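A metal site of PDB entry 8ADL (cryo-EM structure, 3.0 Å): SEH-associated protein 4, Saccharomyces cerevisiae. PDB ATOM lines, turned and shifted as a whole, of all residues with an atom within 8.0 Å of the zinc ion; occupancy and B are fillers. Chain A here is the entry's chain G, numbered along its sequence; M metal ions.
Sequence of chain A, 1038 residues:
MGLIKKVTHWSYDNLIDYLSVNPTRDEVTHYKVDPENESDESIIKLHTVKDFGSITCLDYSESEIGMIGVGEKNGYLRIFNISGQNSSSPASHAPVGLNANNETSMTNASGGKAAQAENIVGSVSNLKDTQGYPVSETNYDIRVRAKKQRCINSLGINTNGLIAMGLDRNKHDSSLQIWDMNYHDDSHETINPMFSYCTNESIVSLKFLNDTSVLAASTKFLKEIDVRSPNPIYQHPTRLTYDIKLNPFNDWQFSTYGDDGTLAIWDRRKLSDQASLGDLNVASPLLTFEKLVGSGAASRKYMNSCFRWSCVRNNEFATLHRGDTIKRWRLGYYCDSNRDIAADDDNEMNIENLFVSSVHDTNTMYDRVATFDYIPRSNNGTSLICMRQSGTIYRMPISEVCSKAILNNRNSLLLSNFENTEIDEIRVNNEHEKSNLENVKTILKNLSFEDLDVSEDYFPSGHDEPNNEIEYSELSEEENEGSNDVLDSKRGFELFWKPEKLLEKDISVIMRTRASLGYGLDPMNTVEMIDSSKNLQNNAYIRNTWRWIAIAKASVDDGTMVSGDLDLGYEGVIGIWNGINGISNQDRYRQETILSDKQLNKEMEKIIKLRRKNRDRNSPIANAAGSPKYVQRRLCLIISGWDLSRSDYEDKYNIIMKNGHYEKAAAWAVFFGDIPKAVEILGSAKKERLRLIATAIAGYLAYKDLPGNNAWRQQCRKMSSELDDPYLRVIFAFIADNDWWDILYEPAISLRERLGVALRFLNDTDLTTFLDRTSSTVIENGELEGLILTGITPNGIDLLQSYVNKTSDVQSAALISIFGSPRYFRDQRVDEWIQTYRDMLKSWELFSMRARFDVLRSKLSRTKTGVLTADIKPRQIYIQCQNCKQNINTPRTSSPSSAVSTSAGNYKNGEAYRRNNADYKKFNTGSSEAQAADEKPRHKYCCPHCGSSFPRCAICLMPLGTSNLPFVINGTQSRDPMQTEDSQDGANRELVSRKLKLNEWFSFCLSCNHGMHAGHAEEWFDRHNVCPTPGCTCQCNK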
ATOM      1  N   GLN A 880      -3.506   0.771 -29.657  1.00  0.00           N
ATOM      2  CA  GLN A 880      -3.187  -0.515 -29.066  1.00  0.00           C
ATOM      3  C   GLN A 880      -4.210  -0.854 -27.981  1.00  0.00           C
ATOM      4  O   GLN A 880      -5.166  -0.124 -27.737  1.00  0.00           O
ATOM      5  CB  GLN A 880      -1.769  -0.509 -28.497  1.00  0.00           C
ATOM      6  CG  GLN A 880      -0.675  -0.414 -29.547  1.00  0.00           C
ATOM      7  CD  GLN A 880       0.706  -0.636 -28.967  1.00  0.00           C
ATOM      8  OE1 GLN A 880       0.905  -0.547 -27.759  1.00  0.00           O
ATOM      9  NE2 GLN A 880       1.675  -0.915 -29.830  1.00  0.00           N
ATOM     10  N   CYS A 881      -3.997  -1.997 -27.310  1.00  0.00           N
ATOM     11  CA  CYS A 881      -4.880  -2.437 -26.238  1.00  0.00           C
ATOM     12  C   CYS A 881      -4.139  -2.902 -24.992  1.00  0.00           C
ATOM     13  O   CYS A 881      -4.803  -3.138 -23.978  1.00  0.00           O
ATOM     14  CB  CYS A 881      -5.807  -3.568 -26.719  1.00  0.00           C
ATOM     15  SG  CYS A 881      -5.025  -5.188 -26.869  1.00  0.00           S
ATOM     16  N   GLN A 882      -2.817  -3.096 -25.057  1.00  0.00           N
ATOM     17  CA  GLN A 882      -1.935  -3.424 -23.938  1.00  0.00           C
ATOM     18  C   GLN A 882      -2.242  -4.795 -23.311  1.00  0.00           C
ATOM     19  O   GLN A 882      -1.683  -5.134 -22.268  1.00  0.00           O
ATOM     20  CB  GLN A 882      -1.950  -2.329 -22.853  1.00  0.00           C
ATOM     21  CG  GLN A 882      -0.613  -2.138 -22.126  1.00  0.00           C
ATOM     22  CD  GLN A 882      -0.710  -1.114 -21.006  1.00  0.00           C
ATOM     23  OE1 GLN A 882      -1.785  -0.622 -20.699  1.00  0.00           O
ATOM     24  NE2 GLN A 882       0.434  -0.808 -20.397  1.00  0.00           N
ATOM     25  N   ASN A 883      -3.102  -5.595 -23.938  1.00  0.00           N
ATOM     26  CA  ASN A 883      -3.363  -6.961 -23.539  1.00  0.00           C
ATOM     27  C   ASN A 883      -2.835  -7.981 -24.528  1.00  0.00           C
ATOM     28  O   ASN A 883      -2.382  -9.054 -24.128  1.00  0.00           O
ATOM     29  CB  ASN A 883      -4.870  -7.181 -23.338  1.00  0.00           C
ATOM     30  CG  ASN A 883      -5.352  -6.721 -21.972  1.00  0.00           C
ATOM     31  OD1 ASN A 883      -6.308  -5.953 -21.868  1.00  0.00           O
ATOM     32  ND2 ASN A 883      -4.685  -7.197 -20.925  1.00  0.00           N
ATOM     33  N   CYS A 884      -2.870  -7.664 -25.827  1.00  0.00           N
ATOM     34  CA  CYS A 884      -2.119  -8.392 -26.827  1.00  0.00           C
ATOM     35  C   CYS A 884      -1.167  -7.489 -27.620  1.00  0.00           C
ATOM     36  O   CYS A 884      -0.431  -7.999 -28.464  1.00  0.00           O
ATOM     37  CB  CYS A 884      -3.065  -9.113 -27.787  1.00  0.00           C
ATOM     38  SG  CYS A 884      -3.987  -8.042 -28.908  1.00  0.00           S
ATOM     39  N   LYS A 885      -1.175  -6.176 -27.347  1.00  0.00           N
ATOM     40  CA  LYS A 885      -0.291  -5.191 -27.962  1.00  0.00           C
ATOM     41  C   LYS A 885      -0.395  -5.198 -29.487  1.00  0.00           C
ATOM     42  O   LYS A 885       0.601  -5.225 -30.212  1.00  0.00           O
ATOM     43  CB  LYS A 885       1.160  -5.397 -27.522  1.00  0.00           C
ATOM     44  CG  LYS A 885       1.412  -5.105 -26.052  1.00  0.00           C
ATOM     45  CD  LYS A 885       2.833  -5.446 -25.657  1.00  0.00           C
ATOM     46  CE  LYS A 885       3.064  -5.203 -24.165  1.00  0.00           C
ATOM     47  NZ  LYS A 885       4.445  -5.569 -23.752  1.00  0.00           N
ATOM     48  N   GLN A 886      -1.632  -5.162 -29.983  1.00  0.00           N
ATOM     49  CA  GLN A 886      -1.915  -5.137 -31.409  1.00  0.00           C
ATOM     50  C   GLN A 886      -2.923  -4.040 -31.711  1.00  0.00           C
ATOM     51  O   GLN A 886      -3.483  -3.416 -30.808  1.00  0.00           O
ATOM     52  CB  GLN A 886      -2.458  -6.494 -31.901  1.00  0.00           C
ATOM     53  CG  GLN A 886      -1.481  -7.649 -31.772  1.00  0.00           C
ATOM     54  CD  GLN A 886      -0.464  -7.680 -32.895  1.00  0.00           C
ATOM     55  OE1 GLN A 886      -0.816  -7.567 -34.070  1.00  0.00           O
ATOM     56  NE2 GLN A 886       0.802  -7.856 -32.542  1.00  0.00           N
ATOM     57  N   ASN A 887      -3.134  -3.810 -33.004  1.00  0.00           N
ATOM     58  CA  ASN A 887      -4.144  -2.858 -33.441  1.00  0.00           C
ATOM     59  C   ASN A 887      -5.527  -3.403 -33.163  1.00  0.00           C
ATOM     60  O   ASN A 887      -5.783  -4.603 -33.310  1.00  0.00           O
ATOM     61  CB  ASN A 887      -3.968  -2.552 -34.928  1.00  0.00           C
ATOM     62  CG  ASN A 887      -4.573  -1.215 -35.320  1.00  0.00           C
ATOM     63  OD1 ASN A 887      -5.080  -0.474 -34.473  1.00  0.00           O
ATOM     64  ND2 ASN A 887      -4.521  -0.890 -36.609  1.00  0.00           N
ATOM     65  N   ILE A 888      -6.451  -2.523 -32.748  1.00  0.00           N
ATOM     66  CA  ILE A 888      -7.802  -2.962 -32.438  1.00  0.00           C
ATOM     67  C   ILE A 888      -8.723  -2.908 -33.652  1.00  0.00           C
ATOM     68  O   ILE A 888      -9.894  -3.313 -33.549  1.00  0.00           O
ATOM     69  CB  ILE A 888      -8.430  -2.117 -31.305  1.00  0.00           C
ATOM     70  CG1 ILE A 888      -8.834  -0.742 -31.827  1.00  0.00           C
ATOM     71  CG2 ILE A 888      -7.448  -1.985 -30.153  1.00  0.00           C
ATOM     72  CD1 ILE A 888      -9.823  -0.036 -30.935  1.00  0.00           C
ATOM     73  N   CYS A 942     -15.091  -5.390 -28.211  1.00  0.00           N
ATOM     74  CA  CYS A 942     -14.000  -6.187 -27.657  1.00  0.00           C
ATOM     75  C   CYS A 942     -12.829  -6.146 -28.627  1.00  0.00           C
ATOM     76  O   CYS A 942     -12.987  -5.807 -29.810  1.00  0.00           O
ATOM     77  CB  CYS A 942     -14.423  -7.635 -27.401  1.00  0.00           C
ATOM     78  SG  CYS A 942     -15.295  -7.896 -25.851  1.00  0.00           S
ATOM     79  N   CYS A 943     -11.647  -6.468 -28.119  1.00  0.00           N
ATOM     80  CA  CYS A 943     -10.469  -6.504 -28.983  1.00  0.00           C
ATOM     81  C   CYS A 943     -10.557  -7.702 -29.926  1.00  0.00           C
ATOM     82  O   CYS A 943     -10.855  -8.813 -29.477  1.00  0.00           O
ATOM     83  CB  CYS A 943      -9.190  -6.592 -28.140  1.00  0.00           C
ATOM     84  SG  CYS A 943      -7.677  -6.793 -29.110  1.00  0.00           S
ATOM     85  N   PRO A 944     -10.316  -7.515 -31.222  1.00  0.00           N
ATOM     86  CA  PRO A 944     -10.446  -8.616 -32.178  1.00  0.00           C
ATOM     87  C   PRO A 944      -9.274  -9.600 -32.187  1.00  0.00           C
ATOM     88  O   PRO A 944      -9.274 -10.512 -33.015  1.00  0.00           O
ATOM     89  CB  PRO A 944     -10.548  -7.892 -33.541  1.00  0.00           C
ATOM     90  CG  PRO A 944     -10.773  -6.450 -33.203  1.00  0.00           C
ATOM     91  CD  PRO A 944     -10.085  -6.233 -31.899  1.00  0.00           C
ATOM     92  N   HIS A 945      -8.295  -9.436 -31.300  1.00  0.00           N
ATOM     93  CA  HIS A 945      -7.183 -10.374 -31.239  1.00  0.00           C
ATOM     94  C   HIS A 945      -6.989 -11.041 -29.873  1.00  0.00           C
ATOM     95  O   HIS A 945      -6.351 -12.094 -29.817  1.00  0.00           O
ATOM     96  CB  HIS A 945      -5.865  -9.664 -31.612  1.00  0.00           C
ATOM     97  CG  HIS A 945      -5.838  -9.149 -33.013  1.00  0.00           C
ATOM     98  ND1 HIS A 945      -6.607  -9.691 -34.024  1.00  0.00           N
ATOM     99  CD2 HIS A 945      -5.144  -8.129 -33.578  1.00  0.00           C
ATOM    100  CE1 HIS A 945      -6.375  -9.036 -35.145  1.00  0.00           C
ATOM    101  NE2 HIS A 945      -5.491  -8.080 -34.904  1.00  0.00           N
ATOM    102  N   CYS A 946      -7.519 -10.459 -28.795  1.00  0.00           N
ATOM    103  CA  CYS A 946      -7.420 -11.099 -27.487  1.00  0.00           C
ATOM    104  C   CYS A 946      -8.720 -11.062 -26.696  1.00  0.00           C
ATOM    105  O   CYS A 946      -8.761 -11.632 -25.605  1.00  0.00           O
ATOM    106  CB  CYS A 946      -6.298 -10.447 -26.658  1.00  0.00           C
ATOM    107  SG  CYS A 946      -6.596  -8.728 -26.176  1.00  0.00           S
ATOM    108  N   GLY A 947      -9.765 -10.406 -27.200  1.00  0.00           N
ATOM    109  CA  GLY A 947     -11.060 -10.434 -26.560  1.00  0.00           C
ATOM    110  C   GLY A 947     -11.187  -9.584 -25.303  1.00  0.00           C
ATOM    111  O   GLY A 947     -12.210  -9.662 -24.631  1.00  0.00           O
ATOM    112  N   SER A 948     -10.168  -8.803 -24.976  1.00  0.00           N
ATOM    113  CA  SER A 948     -10.218  -7.982 -23.770  1.00  0.00           C
ATOM    114  C   SER A 948     -11.208  -6.833 -23.948  1.00  0.00           C
ATOM    115  O   SER A 948     -11.494  -6.397 -25.071  1.00  0.00           O
ATOM    116  CB  SER A 948      -8.832  -7.425 -23.439  1.00  0.00           C
ATOM    117  OG  SER A 948      -8.851  -6.699 -22.228  1.00  0.00           O
ATOM    118  N   SER A 949     -11.743  -6.353 -22.836  1.00  0.00           N
ATOM    119  CA  SER A 949     -12.803  -5.361 -22.885  1.00  0.00           C
ATOM    120  C   SER A 949     -12.254  -3.988 -23.220  1.00  0.00           C
ATOM    121  O   SER A 949     -11.222  -3.572 -22.699  1.00  0.00           O
ATOM    122  CB  SER A 949     -13.542  -5.309 -21.540  1.00  0.00           C
ATOM    123  OG  SER A 949     -14.249  -6.514 -21.296  1.00  0.00           O
ATOM    124  N   PHE A 950     -12.958  -3.292 -24.116  1.00  0.00           N
ATOM    125  CA  PHE A 950     -12.583  -1.943 -24.472  1.00  0.00           C
ATOM    126  C   PHE A 950     -12.969  -0.980 -23.347  1.00  0.00           C
ATOM    127  O   PHE A 950     -13.923  -1.233 -22.603  1.00  0.00           O
ATOM    128  CB  PHE A 950     -13.259  -1.515 -25.768  1.00  0.00           C
ATOM    129  CG  PHE A 950     -12.583  -2.030 -27.000  1.00  0.00           C
ATOM    130  CD1 PHE A 950     -11.281  -2.509 -26.959  1.00  0.00           C
ATOM    131  CD2 PHE A 950     -13.253  -2.040 -28.220  1.00  0.00           C
ATOM    132  CE1 PHE A 950     -10.657  -2.980 -28.093  1.00  0.00           C
ATOM    133  CE2 PHE A 950     -12.632  -2.511 -29.363  1.00  0.00           C
ATOM    134  CZ  PHE A 950     -11.331  -2.981 -29.290  1.00  0.00           C
HETATM  135 ZN    ZN M   1      -5.816  -7.189 -27.755  1.00  0.00          ZN
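The backbone NH (N) of Asn 883 lies close to the side-chain sulfur (SG) of Cys 881, at 3.5 Å. N of His 945 lies close to SG of Cys 943 (3.5 Å). The backbone NH (N) of Cys 943 is in hydrogen-bond range of the backbone carbonyl oxygen (O) of Ser 948. The backbone NH (N) of Ser 948 lies close to the side-chain sulfur (SG) of Cys 946 (3.8 Å).
Within 4 Å of the zinc ion: Cys 881, Cys 884, Cys 943 and Cys 946. Along chain A the residues within 4 Å of the zinc ion span positions 881 to 946.
The zinc ion is bound by SG of Cys 884. SG of Cys 881 is bound to the zinc ion. SG of Cys 943 binds the zinc ion (2.3 Å). The side-chain sulfur (SG) of Cys 946 binds the zinc ion (2.3 Å).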
